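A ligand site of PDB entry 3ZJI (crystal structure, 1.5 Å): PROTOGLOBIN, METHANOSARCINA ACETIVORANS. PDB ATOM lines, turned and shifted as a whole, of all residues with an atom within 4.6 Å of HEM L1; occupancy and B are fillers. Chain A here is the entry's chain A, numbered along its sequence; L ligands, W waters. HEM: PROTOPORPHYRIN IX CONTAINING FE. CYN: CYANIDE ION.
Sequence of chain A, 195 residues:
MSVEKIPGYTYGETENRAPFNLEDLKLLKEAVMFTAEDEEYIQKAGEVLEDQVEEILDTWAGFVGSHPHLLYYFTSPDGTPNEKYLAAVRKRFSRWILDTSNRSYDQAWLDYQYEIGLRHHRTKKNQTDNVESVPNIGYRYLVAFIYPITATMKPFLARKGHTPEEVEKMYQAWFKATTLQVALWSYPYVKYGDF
Water W3 bridges O2D of HEM L1 (2.7 Å) and OG1 of Thr 128 (2.7 Å).
Water W1 lies within hydrogen-bond range of an oxygen (O2A) of HEM L1 and the guanidinium group of Arg 92.
Water W2 bridges O1A of HEM L1 and O of Arg 92.
Water W4 bridges an oxygen (O1D) of HEM L1 (3.0 Å) and the backbone NH of Thr 128 (3.3 Å).
N of Asn 126 lies within hydrogen-bond range of O1D of HEM L1, 2.8 Å away.
The side-chain hydroxyl of Tyr 85 sits at hydrogen-bond distance from an oxygen (O1D) of HEM L1 (2.6 Å).
FE of HEM L1 is bound by NE2 of His 120, 2.1 Å away.
OH of Tyr 112 sits at hydrogen-bond distance from O1A of HEM L1, 2.7 Å away.
An oxygen (O2A) of HEM L1 lies within salt-bridge range of the guanidinium group (NE) of Arg 92, 2.9 Å away.
NH1 of Arg 119 is in salt-bridge range of O2A of HEM L1 (2.8 Å).
Merely in contact with HEM L1: Phe 145, Trp 96, Tyr 141, Leu 70, Val 182, Trp 185, Phe 74, Val 89, Phe 93, Tyr 73, Lys 125, Ile 137, Leu 142, Ile 146, Ile 149, Ile 116 and Thr 178.
Hydrophobic or aromatic side chains within 4 Å of HEM L1: Tyr 73, Phe 74, Tyr 85, Val 89, Phe 93, Trp 96, Tyr 112, Ile 116, His 120, Ile 137, Tyr 141, Phe 145, Ile 149, Val 182 and Trp 185.
Within 4 Å of HEM L1: Leu 70, Tyr 73, Phe 74, Tyr 85, Val 89, Arg 92, Phe 93, Trp 96, Tyr 112, Ile 116, Arg 119, His 120, Lys 125, Asn 126, Ile 137, Tyr 141, Leu 142, Phe 145, Ile 146, Ile 149, Thr 178, Val 182 and Trp 185.
The side-chain hydroxyl (OH) of Tyr 85 sits at hydrogen-bond distance from the side-chain amide oxygen (OD1) of Asn 126 (3.1 Å).
N of Lys 125 lies close to O of Arg 119 (3.5 Å).
The side-chain hydroxyl (OH) of Tyr 112 sits at hydrogen-bond distance from the guanidinium group (NH1) of Arg 119, at 3.4 Å.
The side-chain hydroxyl (OH) of Tyr 85 lies within hydrogen-bond range of the side-chain amino group (NZ) of Lys 125, 2.9 Å away.
A ring nitrogen (ND1) of His 120 lies within hydrogen-bond range of the backbone carbonyl oxygen (O) of Ile 116, at 3.0 Å.
The side-chain amide oxygen (OD1) of Asn 126 lies within hydrogen-bond range of the side-chain amino group (NZ) of Lys 125.
N of Ile 137 is in hydrogen-bond range of O of His 120, 3.2 Å away.
The side-chain hydroxyl (OG1) of Thr 128 sits at hydrogen-bond distance from the guanidinium group (NE) of Arg 119 (3.3 Å).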
ATOM      1  N   TYR A   9      -0.847 -24.604  33.246  1.00  0.00           N
ATOM      2  CA  TYR A   9      -1.717 -24.172  32.163  1.00  0.00           C
ATOM      3  C   TYR A   9      -2.793 -23.257  32.700  1.00  0.00           C
ATOM      4  O   TYR A   9      -3.680 -23.706  33.424  1.00  0.00           O
ATOM      5  CB  TYR A   9      -2.333 -25.381  31.464  1.00  0.00           C
ATOM      6  CG  TYR A   9      -3.244 -25.049  30.306  1.00  0.00           C
ATOM      7  CD1 TYR A   9      -2.737 -24.552  29.109  1.00  0.00           C
ATOM      8  CD2 TYR A   9      -4.615 -25.268  30.405  1.00  0.00           C
ATOM      9  CE1 TYR A   9      -3.586 -24.262  28.035  1.00  0.00           C
ATOM     10  CE2 TYR A   9      -5.465 -24.993  29.348  1.00  0.00           C
ATOM     11  CZ  TYR A   9      -4.948 -24.505  28.168  1.00  0.00           C
ATOM     12  OH  TYR A   9      -5.804 -24.253  27.120  1.00  0.00           O
ATOM     13  N   VAL A  64      14.242 -30.762  18.812  1.00  0.00           N
ATOM     14  CA  VAL A  64      14.869 -29.908  19.812  1.00  0.00           C
ATOM     15  C   VAL A  64      16.101 -30.601  20.392  1.00  0.00           C
ATOM     16  O   VAL A  64      17.164 -29.983  20.538  1.00  0.00           O
ATOM     17  CB  VAL A  64      13.874 -29.524  20.906  1.00  0.00           C
ATOM     18  CG1 VAL A  64      14.591 -28.825  22.055  1.00  0.00           C
ATOM     19  CG2 VAL A  64      12.761 -28.649  20.320  1.00  0.00           C
ATOM     20  N   LEU A  70      19.807 -25.900  20.851  1.00  0.00           N
ATOM     21  CA  LEU A  70      18.358 -25.819  21.027  1.00  0.00           C
ATOM     22  C   LEU A  70      17.952 -26.481  22.333  1.00  0.00           C
ATOM     23  O   LEU A  70      17.254 -25.876  23.149  1.00  0.00           O
ATOM     24  CB  LEU A  70      17.619 -26.422  19.825  1.00  0.00           C
ATOM     25  CG  LEU A  70      17.983 -25.750  18.488  1.00  0.00           C
ATOM     26  CD1 LEU A  70      17.218 -26.393  17.339  1.00  0.00           C
ATOM     27  CD2 LEU A  70      17.768 -24.232  18.523  1.00  0.00           C
ATOM     28  N   TYR A  73      17.986 -24.711  25.901  1.00  0.00           N
ATOM     29  CA  TYR A  73      16.984 -23.893  26.583  1.00  0.00           C
ATOM     30  C   TYR A  73      16.181 -24.644  27.637  1.00  0.00           C
ATOM     31  O   TYR A  73      15.488 -24.017  28.444  1.00  0.00           O
ATOM     32  CB  TYR A  73      16.087 -23.160  25.566  1.00  0.00           C
ATOM     33  CG  TYR A  73      16.911 -22.193  24.755  1.00  0.00           C
ATOM     34  CD1 TYR A  73      17.374 -21.015  25.328  1.00  0.00           C
ATOM     35  CD2 TYR A  73      17.307 -22.488  23.451  1.00  0.00           C
ATOM     36  CE1 TYR A  73      18.196 -20.140  24.610  1.00  0.00           C
ATOM     37  CE2 TYR A  73      18.137 -21.627  22.727  1.00  0.00           C
ATOM     38  CZ  TYR A  73      18.574 -20.450  23.315  1.00  0.00           C
ATOM     39  OH  TYR A  73      19.396 -19.585  22.637  1.00  0.00           O
ATOM     40  N   PHE A  74      16.307 -25.979  27.635  1.00  0.00           N
ATOM     41  CA  PHE A  74      15.693 -26.843  28.652  1.00  0.00           C
ATOM     42  C   PHE A  74      16.715 -27.386  29.654  1.00  0.00           C
ATOM     43  O   PHE A  74      16.375 -28.249  30.486  1.00  0.00           O
ATOM     44  CB  PHE A  74      14.995 -28.033  27.993  1.00  0.00           C
ATOM     45  CG  PHE A  74      13.731 -27.676  27.265  1.00  0.00           C
ATOM     46  CD1 PHE A  74      12.525 -27.606  27.939  1.00  0.00           C
ATOM     47  CD2 PHE A  74      13.765 -27.401  25.898  1.00  0.00           C
ATOM     48  CE1 PHE A  74      11.346 -27.311  27.255  1.00  0.00           C
ATOM     49  CE2 PHE A  74      12.582 -27.098  25.208  1.00  0.00           C
ATOM     50  CZ  PHE A  74      11.388 -27.049  25.882  1.00  0.00           C
ATOM     51  N   TYR A  85      11.384 -30.365  33.609  1.00  0.00           N
ATOM     52  CA  TYR A  85      11.036 -29.202  32.800  1.00  0.00           C
ATOM     53  C   TYR A  85      10.503 -29.655  31.441  1.00  0.00           C
ATOM     54  O   TYR A  85       9.418 -29.239  31.024  1.00  0.00           O
ATOM     55  CB  TYR A  85      12.308 -28.373  32.619  1.00  0.00           C
ATOM     56  CG  TYR A  85      12.191 -26.975  32.039  1.00  0.00           C
ATOM     57  CD1 TYR A  85      11.011 -26.228  32.072  1.00  0.00           C
ATOM     58  CD2 TYR A  85      13.338 -26.348  31.554  1.00  0.00           C
ATOM     59  CE1 TYR A  85      10.970 -24.915  31.580  1.00  0.00           C
ATOM     60  CE2 TYR A  85      13.318 -25.043  31.057  1.00  0.00           C
ATOM     61  CZ  TYR A  85      12.139 -24.337  31.070  1.00  0.00           C
ATOM     62  OH  TYR A  85      12.168 -23.043  30.618  1.00  0.00           O
ATOM     63  N   VAL A  89       6.556 -28.999  30.206  1.00  0.00           N
ATOM     64  CA  VAL A  89       6.320 -28.201  29.015  1.00  0.00           C
ATOM     65  C   VAL A  89       5.633 -29.049  27.951  1.00  0.00           C
ATOM     66  O   VAL A  89       4.742 -28.552  27.255  1.00  0.00           O
ATOM     67  CB  VAL A  89       7.618 -27.574  28.491  1.00  0.00           C
ATOM     68  CG1 VAL A  89       7.388 -26.899  27.146  1.00  0.00           C
ATOM     69  CG2 VAL A  89       8.189 -26.580  29.519  1.00  0.00           C
ATOM     70  N   ARG A  92       1.953 -28.908  28.290  1.00  0.00           N
ATOM     71  CA  ARG A  92       1.368 -27.640  27.856  1.00  0.00           C
ATOM     72  C   ARG A  92       1.454 -27.454  26.337  1.00  0.00           C
ATOM     73  O   ARG A  92       0.558 -26.865  25.734  1.00  0.00           O
ATOM     74  CB  ARG A  92       1.961 -26.451  28.633  1.00  0.00           C
ATOM     75  CG  ARG A  92       1.690 -26.548  30.136  1.00  0.00           C
ATOM     76  CD  ARG A  92       1.936 -25.237  30.878  1.00  0.00           C
ATOM     77  NE  ARG A  92       3.335 -24.845  30.835  1.00  0.00           N
ATOM     78  CZ  ARG A  92       4.280 -25.268  31.670  1.00  0.00           C
ATOM     79  NH1 ARG A  92       3.993 -26.128  32.652  1.00  0.00           N
ATOM     80  NH2 ARG A  92       5.533 -24.837  31.517  1.00  0.00           N
ATOM     81  N   PHE A  93       2.521 -27.953  25.742  1.00  0.00           N
ATOM     82  CA  PHE A  93       2.672 -27.900  24.289  1.00  0.00           C
ATOM     83  C   PHE A  93       1.584 -28.764  23.629  1.00  0.00           C
ATOM     84  O   PHE A  93       0.989 -28.377  22.621  1.00  0.00           O
ATOM     85  CB  PHE A  93       4.074 -28.377  23.894  1.00  0.00           C
ATOM     86  CG  PHE A  93       4.416 -28.199  22.438  1.00  0.00           C
ATOM     87  CD1 PHE A  93       3.922 -29.064  21.466  1.00  0.00           C
ATOM     88  CD2 PHE A  93       5.303 -27.206  22.037  1.00  0.00           C
ATOM     89  CE1 PHE A  93       4.256 -28.931  20.135  1.00  0.00           C
ATOM     90  CE2 PHE A  93       5.643 -27.051  20.695  1.00  0.00           C
ATOM     91  CZ  PHE A  93       5.138 -27.932  19.745  1.00  0.00           C
ATOM     92  N   TRP A  96      -1.466 -26.838  23.559  1.00  0.00           N
ATOM     93  CA  TRP A  96      -1.367 -25.770  22.580  1.00  0.00           C
ATOM     94  C   TRP A  96      -1.732 -26.251  21.170  1.00  0.00           C
ATOM     95  O   TRP A  96      -2.324 -25.512  20.402  1.00  0.00           O
ATOM     96  CB  TRP A  96       0.047 -25.183  22.593  1.00  0.00           C
ATOM     97  CG  TRP A  96       0.350 -24.283  21.440  1.00  0.00           C
ATOM     98  CD1 TRP A  96       0.026 -22.957  21.318  1.00  0.00           C
ATOM     99  CD2 TRP A  96       1.004 -24.638  20.219  1.00  0.00           C
ATOM    100  NE1 TRP A  96       0.451 -22.473  20.118  1.00  0.00           N
ATOM    101  CE2 TRP A  96       1.037 -23.488  19.408  1.00  0.00           C
ATOM    102  CE3 TRP A  96       1.558 -25.824  19.726  1.00  0.00           C
ATOM    103  CZ2 TRP A  96       1.630 -23.470  18.138  1.00  0.00           C
ATOM    104  CZ3 TRP A  96       2.151 -25.819  18.455  1.00  0.00           C
ATOM    105  CH2 TRP A  96       2.181 -24.644  17.681  1.00  0.00           C
ATOM    106  N   TYR A 112      -3.558 -15.341  26.524  1.00  0.00           N
ATOM    107  CA  TYR A 112      -2.650 -16.452  26.684  1.00  0.00           C
ATOM    108  C   TYR A 112      -1.448 -16.360  25.730  1.00  0.00           C
ATOM    109  O   TYR A 112      -0.373 -16.798  26.070  1.00  0.00           O
ATOM    110  CB  TYR A 112      -3.364 -17.815  26.570  1.00  0.00           C
ATOM    111  CG  TYR A 112      -2.625 -18.883  27.358  1.00  0.00           C
ATOM    112  CD1 TYR A 112      -2.493 -18.787  28.748  1.00  0.00           C
ATOM    113  CD2 TYR A 112      -2.014 -19.959  26.709  1.00  0.00           C
ATOM    114  CE1 TYR A 112      -1.792 -19.730  29.477  1.00  0.00           C
ATOM    115  CE2 TYR A 112      -1.298 -20.931  27.444  1.00  0.00           C
ATOM    116  CZ  TYR A 112      -1.187 -20.805  28.816  1.00  0.00           C
ATOM    117  OH  TYR A 112      -0.516 -21.741  29.555  1.00  0.00           O
ATOM    118  N   ILE A 116       2.347 -16.853  26.812  1.00  0.00           N
ATOM    119  CA  ILE A 116       3.317 -17.770  26.231  1.00  0.00           C
ATOM    120  C   ILE A 116       4.575 -17.013  25.782  1.00  0.00           C
ATOM    121  O   ILE A 116       5.699 -17.493  25.984  1.00  0.00           O
ATOM    122  CB  ILE A 116       2.741 -18.568  25.041  1.00  0.00           C
ATOM    123  CG1 ILE A 116       1.596 -19.478  25.519  1.00  0.00           C
ATOM    124  CG2 ILE A 116       3.845 -19.395  24.357  1.00  0.00           C
ATOM    125  CD1 ILE A 116       0.805 -20.121  24.385  1.00  0.00           C
ATOM    126  N   ARG A 119       6.675 -16.357  28.797  1.00  0.00           N
ATOM    127  CA  ARG A 119       7.305 -17.587  29.290  1.00  0.00           C
ATOM    128  C   ARG A 119       8.534 -18.024  28.499  1.00  0.00           C
ATOM    129  O   ARG A 119       9.415 -18.669  29.073  1.00  0.00           O
ATOM    130  CB  ARG A 119       6.299 -18.733  29.379  1.00  0.00           C
ATOM    131  CG  ARG A 119       5.253 -18.517  30.456  1.00  0.00           C
ATOM    132  CD  ARG A 119       4.225 -19.637  30.488  1.00  0.00           C
ATOM    133  NE  ARG A 119       3.173 -19.343  31.459  1.00  0.00           N
ATOM    134  CZ  ARG A 119       2.297 -20.220  31.922  1.00  0.00           C
ATOM    135  NH1 ARG A 119       2.276 -21.464  31.472  1.00  0.00           N
ATOM    136  NH2 ARG A 119       1.404 -19.846  32.833  1.00  0.00           N
ATOM    137  N   HIS A 120       8.586 -17.698  27.207  1.00  0.00           N
ATOM    138  CA  HIS A 120       9.815 -17.945  26.424  1.00  0.00           C
ATOM    139  C   HIS A 120      10.841 -16.880  26.766  1.00  0.00           C
ATOM    140  O   HIS A 120      12.039 -17.166  26.825  1.00  0.00           O
ATOM    141  CB  HIS A 120       9.534 -17.939  24.923  1.00  0.00           C
ATOM    142  CG  HIS A 120       8.865 -19.190  24.431  1.00  0.00           C
ATOM    143  ND1 HIS A 120       7.502 -19.410  24.541  1.00  0.00           N
ATOM    144  CD2 HIS A 120       9.378 -20.289  23.830  1.00  0.00           C
ATOM    145  CE1 HIS A 120       7.211 -20.586  24.008  1.00  0.00           C
ATOM    146  NE2 HIS A 120       8.331 -21.148  23.581  1.00  0.00           N
ATOM    147  N   LYS A 125      10.307 -16.903  31.929  1.00  0.00           N
ATOM    148  CA  LYS A 125      10.919 -18.232  31.728  1.00  0.00           C
ATOM    149  C   LYS A 125      11.356 -18.852  33.054  1.00  0.00           C
ATOM    150  O   LYS A 125      11.884 -18.158  33.936  1.00  0.00           O
ATOM    151  CB  LYS A 125      12.101 -18.174  30.758  1.00  0.00           C
ATOM    152  CG  LYS A 125      12.539 -19.574  30.315  1.00  0.00           C
ATOM    153  CD  LYS A 125      13.734 -19.519  29.387  1.00  0.00           C
ATOM    154  CE  LYS A 125      14.153 -20.911  28.932  1.00  0.00           C
ATOM    155  NZ  LYS A 125      14.711 -21.732  30.057  1.00  0.00           N
ATOM    156  N   ASN A 126      11.098 -20.155  33.189  1.00  0.00           N
ATOM    157  CA  ASN A 126      11.476 -20.996  34.344  1.00  0.00           C
ATOM    158  C   ASN A 126      10.646 -20.791  35.614  1.00  0.00           C
ATOM    159  O   ASN A 126      10.883 -21.455  36.611  1.00  0.00           O
ATOM    160  CB  ASN A 126      12.920 -20.748  34.811  1.00  0.00           C
ATOM    161  CG  ASN A 126      13.898 -20.809  33.664  1.00  0.00           C
ATOM    162  OD1 ASN A 126      13.880 -21.736  32.853  1.00  0.00           O
ATOM    163  ND2 ASN A 126      14.780 -19.811  33.593  1.00  0.00           N
ATOM    164  N   THR A 128       7.151 -20.977  35.737  1.00  0.00           N
ATOM    165  CA  THR A 128       5.937 -21.775  35.763  1.00  0.00           C
ATOM    166  C   THR A 128       6.194 -23.130  36.405  1.00  0.00           C
ATOM    167  O   THR A 128       5.385 -23.623  37.221  1.00  0.00           O
ATOM    168  CB  THR A 128       5.351 -21.926  34.345  1.00  0.00           C
ATOM    169  OG1 THR A 128       5.025 -20.621  33.821  1.00  0.00           O
ATOM    170  CG2 THR A 128       4.103 -22.798  34.327  1.00  0.00           C
ATOM    171  N   ILE A 137      15.110 -17.329  26.133  1.00  0.00           N
ATOM    172  CA  ILE A 137      15.259 -17.952  24.807  1.00  0.00           C
ATOM    173  C   ILE A 137      15.457 -16.860  23.780  1.00  0.00           C
ATOM    174  O   ILE A 137      14.563 -16.047  23.530  1.00  0.00           O
ATOM    175  CB  ILE A 137      14.030 -18.806  24.443  1.00  0.00           C
ATOM    176  CG1 ILE A 137      13.783 -19.880  25.525  1.00  0.00           C
ATOM    177  CG2 ILE A 137      14.263 -19.484  23.080  1.00  0.00           C
ATOM    178  CD1 ILE A 137      12.437 -20.566  25.407  1.00  0.00           C
ATOM    179  N   TYR A 141      15.512 -17.552  17.640  1.00  0.00           N
ATOM    180  CA  TYR A 141      15.037 -18.933  17.517  1.00  0.00           C
ATOM    181  C   TYR A 141      13.517 -19.079  17.520  1.00  0.00           C
ATOM    182  O   TYR A 141      12.985 -20.004  16.901  1.00  0.00           O
ATOM    183  CB  TYR A 141      15.689 -19.835  18.581  1.00  0.00           C
ATOM    184  CG  TYR A 141      17.186 -19.946  18.407  1.00  0.00           C
ATOM    185  CD1 TYR A 141      17.727 -20.458  17.223  1.00  0.00           C
ATOM    186  CD2 TYR A 141      18.056 -19.499  19.389  1.00  0.00           C
ATOM    187  CE1 TYR A 141      19.099 -20.516  17.035  1.00  0.00           C
ATOM    188  CE2 TYR A 141      19.438 -19.580  19.218  1.00  0.00           C
ATOM    189  CZ  TYR A 141      19.949 -20.099  18.042  1.00  0.00           C
ATOM    190  OH  TYR A 141      21.308 -20.151  17.871  1.00  0.00           O
ATOM    191  N   LEU A 142      12.802 -18.172  18.182  1.00  0.00           N
ATOM    192  CA  LEU A 142      11.336 -18.192  18.106  1.00  0.00           C
ATOM    193  C   LEU A 142      10.878 -18.024  16.664  1.00  0.00           C
ATOM    194  O   LEU A 142      10.010 -18.756  16.191  1.00  0.00           O
ATOM    195  CB  LEU A 142      10.681 -17.141  19.016  1.00  0.00           C
ATOM    196  CG  LEU A 142      10.307 -17.620  20.424  1.00  0.00           C
ATOM    197  CD1 LEU A 142      11.565 -17.925  21.225  1.00  0.00           C
ATOM    198  CD2 LEU A 142       9.509 -16.545  21.131  1.00  0.00           C
ATOM    199  N   PHE A 145      11.754 -21.061  14.530  1.00  0.00           N
ATOM    200  CA  PHE A 145      10.993 -22.281  14.799  1.00  0.00           C
ATOM    201  C   PHE A 145       9.646 -22.321  14.087  1.00  0.00           C
ATOM    202  O   PHE A 145       9.033 -23.363  14.022  1.00  0.00           O
ATOM    203  CB  PHE A 145      10.769 -22.505  16.297  1.00  0.00           C
ATOM    204  CG  PHE A 145      11.867 -23.289  16.980  1.00  0.00           C
ATOM    205  CD1 PHE A 145      13.174 -23.316  16.481  1.00  0.00           C
ATOM    206  CD2 PHE A 145      11.587 -23.972  18.162  1.00  0.00           C
ATOM    207  CE1 PHE A 145      14.184 -24.054  17.153  1.00  0.00           C
ATOM    208  CE2 PHE A 145      12.581 -24.695  18.828  1.00  0.00           C
ATOM    209  CZ  PHE A 145      13.879 -24.723  18.334  1.00  0.00           C
ATOM    210  N   ILE A 146       9.201 -21.202  13.510  1.00  0.00           N
ATOM    211  CA  ILE A 146       8.005 -21.249  12.660  1.00  0.00           C
ATOM    212  C   ILE A 146       8.183 -22.361  11.621  1.00  0.00           C
ATOM    213  O   ILE A 146       7.277 -23.165  11.378  1.00  0.00           O
ATOM    214  CB  ILE A 146       7.764 -19.916  11.925  1.00  0.00           C
ATOM    215  CG1 ILE A 146       7.447 -18.805  12.921  1.00  0.00           C
ATOM    216  CG2 ILE A 146       6.624 -20.049  10.888  1.00  0.00           C
ATOM    217  CD1 ILE A 146       7.478 -17.422  12.319  1.00  0.00           C
ATOM    218  N   ILE A 149       8.155 -26.095  13.162  1.00  0.00           N
ATOM    219  CA  ILE A 149       6.788 -26.416  13.603  1.00  0.00           C
ATOM    220  C   ILE A 149       5.945 -26.877  12.407  1.00  0.00           C
ATOM    221  O   ILE A 149       5.310 -27.934  12.461  1.00  0.00           O
ATOM    222  CB  ILE A 149       6.113 -25.222  14.306  1.00  0.00           C
ATOM    223  CG1 ILE A 149       6.696 -25.036  15.720  1.00  0.00           C
ATOM    224  CG2 ILE A 149       4.587 -25.404  14.317  1.00  0.00           C
ATOM    225  CD1 ILE A 149       6.264 -26.104  16.762  1.00  0.00           C
ATOM    226  N   THR A 178       0.693 -20.334  13.108  1.00  0.00           N
ATOM    227  CA  THR A 178       1.968 -20.371  13.831  1.00  0.00           C
ATOM    228  C   THR A 178       2.699 -19.040  13.695  1.00  0.00           C
ATOM    229  O   THR A 178       3.206 -18.495  14.675  1.00  0.00           O
ATOM    230  CB  THR A 178       2.852 -21.543  13.370  1.00  0.00           C
ATOM    231  OG1 THR A 178       2.148 -22.768  13.597  1.00  0.00           O
ATOM    232  CG2 THR A 178       4.182 -21.584  14.126  1.00  0.00           C
ATOM    233  N   VAL A 182       3.775 -16.426  16.726  1.00  0.00           N
ATOM    234  CA  VAL A 182       5.138 -15.961  16.964  1.00  0.00           C
ATOM    235  C   VAL A 182       5.236 -14.444  16.842  1.00  0.00           C
ATOM    236  O   VAL A 182       5.965 -13.795  17.610  1.00  0.00           O
ATOM    237  CB  VAL A 182       6.151 -16.694  16.086  1.00  0.00           C
ATOM    238  CG1 VAL A 182       7.525 -16.071  16.190  1.00  0.00           C
ATOM    239  CG2 VAL A 182       6.206 -18.169  16.474  1.00  0.00           C
ATOM    240  N   TRP A 185       4.083 -13.222  20.113  1.00  0.00           N
ATOM    241  CA  TRP A 185       5.071 -13.532  21.145  1.00  0.00           C
ATOM    242  C   TRP A 185       6.282 -12.614  21.122  1.00  0.00           C
ATOM    243  O   TRP A 185       7.027 -12.562  22.111  1.00  0.00           O
ATOM    244  CB  TRP A 185       5.514 -15.002  21.087  1.00  0.00           C
ATOM    245  CG  TRP A 185       4.408 -15.999  21.190  1.00  0.00           C
ATOM    246  CD1 TRP A 185       3.068 -15.754  21.341  1.00  0.00           C
ATOM    247  CD2 TRP A 185       4.536 -17.423  21.048  1.00  0.00           C
ATOM    248  NE1 TRP A 185       2.357 -16.931  21.298  1.00  0.00           N
ATOM    249  CE2 TRP A 185       3.232 -17.959  21.107  1.00  0.00           C
ATOM    250  CE3 TRP A 185       5.622 -18.294  20.888  1.00  0.00           C
ATOM    251  CZ2 TRP A 185       2.980 -19.338  21.010  1.00  0.00           C
ATOM    252  CZ3 TRP A 185       5.377 -19.664  20.763  1.00  0.00           C
ATOM    253  CH2 TRP A 185       4.062 -20.173  20.846  1.00  0.00           C
HETATM  254  CHA HEM L   1       7.216 -23.399  26.146  1.00  0.00           C
HETATM  255  CHB HEM L   1       5.487 -23.675  21.594  1.00  0.00           C
HETATM  256  CHC HEM L   1       9.690 -21.653  20.257  1.00  0.00           C
HETATM  257  CHD HEM L   1      11.639 -23.855  24.102  1.00  0.00           C
HETATM  258  C1A HEM L   1       6.339 -23.578  25.083  1.00  0.00           C
HETATM  259  C2A HEM L   1       4.929 -23.851  25.151  1.00  0.00           C
HETATM  260  C3A HEM L   1       4.465 -23.923  23.890  1.00  0.00           C
HETATM  261  C4A HEM L   1       5.564 -23.712  22.981  1.00  0.00           C
HETATM  262  CMA HEM L   1       3.028 -24.186  23.433  1.00  0.00           C
HETATM  263  CAA HEM L   1       4.129 -24.003  26.457  1.00  0.00           C
HETATM  264  CBA HEM L   1       3.313 -22.723  26.683  1.00  0.00           C
HETATM  265  CGA HEM L   1       2.601 -22.743  28.006  1.00  0.00           C
HETATM  266  O1A HEM L   1       1.363 -22.995  28.033  1.00  0.00           O
HETATM  267  O2A HEM L   1       3.294 -22.567  29.051  1.00  0.00           O
HETATM  268  C1B HEM L   1       6.451 -23.088  20.810  1.00  0.00           C
HETATM  269  C2B HEM L   1       6.329 -22.647  19.441  1.00  0.00           C
HETATM  270  C3B HEM L   1       7.485 -22.051  19.088  1.00  0.00           C
HETATM  271  C4B HEM L   1       8.387 -22.098  20.224  1.00  0.00           C
HETATM  272  CMB HEM L   1       5.061 -22.812  18.582  1.00  0.00           C
HETATM  273  CAB HEM L   1       7.868 -21.359  17.765  1.00  0.00           C
HETATM  274  CBB HEM L   1       7.163 -21.423  16.645  1.00  0.00           C
HETATM  275  C1C HEM L   1      10.622 -22.163  21.125  1.00  0.00           C
HETATM  276  C2C HEM L   1      12.063 -22.161  20.960  1.00  0.00           C
HETATM  277  C3C HEM L   1      12.591 -22.833  22.000  1.00  0.00           C
HETATM  278  C4C HEM L   1      11.524 -23.226  22.875  1.00  0.00           C
HETATM  279  CMC HEM L   1      12.841 -21.515  19.797  1.00  0.00           C
HETATM  280  CAC HEM L   1      14.072 -23.170  22.227  1.00  0.00           C
HETATM  281  CBC HEM L   1      14.324 -24.486  22.424  1.00  0.00           C
HETATM  282  C1D HEM L   1      10.670 -23.725  25.070  1.00  0.00           C
HETATM  283  C2D HEM L   1      10.871 -23.732  26.494  1.00  0.00           C
HETATM  284  C3D HEM L   1       9.504 -23.563  27.114  1.00  0.00           C
HETATM  285  C4D HEM L   1       8.575 -23.462  26.015  1.00  0.00           C
HETATM  286  CMD HEM L   1      12.189 -23.886  27.265  1.00  0.00           C
HETATM  287  CAD HEM L   1       9.201 -23.439  28.612  1.00  0.00           C
HETATM  288  CBD HEM L   1       9.301 -21.925  28.932  1.00  0.00           C
HETATM  289  CGD HEM L   1       8.989 -21.684  30.379  1.00  0.00           C
HETATM  290  O1D HEM L   1       9.939 -21.787  31.196  1.00  0.00           O
HETATM  291  O2D HEM L   1       7.795 -21.442  30.724  1.00  0.00           O
HETATM  292  NA  HEM L   1       6.706 -23.502  23.744  1.00  0.00           N
HETATM  293  NB  HEM L   1       7.731 -22.758  21.257  1.00  0.00           N
HETATM  294  NC  HEM L   1      10.326 -22.818  22.302  1.00  0.00           N
HETATM  295  ND  HEM L   1       9.307 -23.550  24.819  1.00  0.00           N
HETATM  296 FE   HEM L   1       8.515 -23.167  23.031  1.00  0.00          FE
HETATM  297  C   CYN L   2       8.769 -25.146  22.583  1.00  0.00           C
HETATM  298  N   CYN L   2       8.870 -26.238  22.370  1.00  0.00           N
HETATM  299  O   HOH W   1       5.923 -22.968  29.401  1.00  0.00           O
HETATM  300  O   HOH W   2      -0.220 -24.130  26.130  1.00  0.00           O
HETATM  301  O   HOH W   3       7.481 -20.009  32.959  1.00  0.00           O
HETATM  302  O   HOH W   4       8.814 -22.996  33.671  1.00  0.00           O
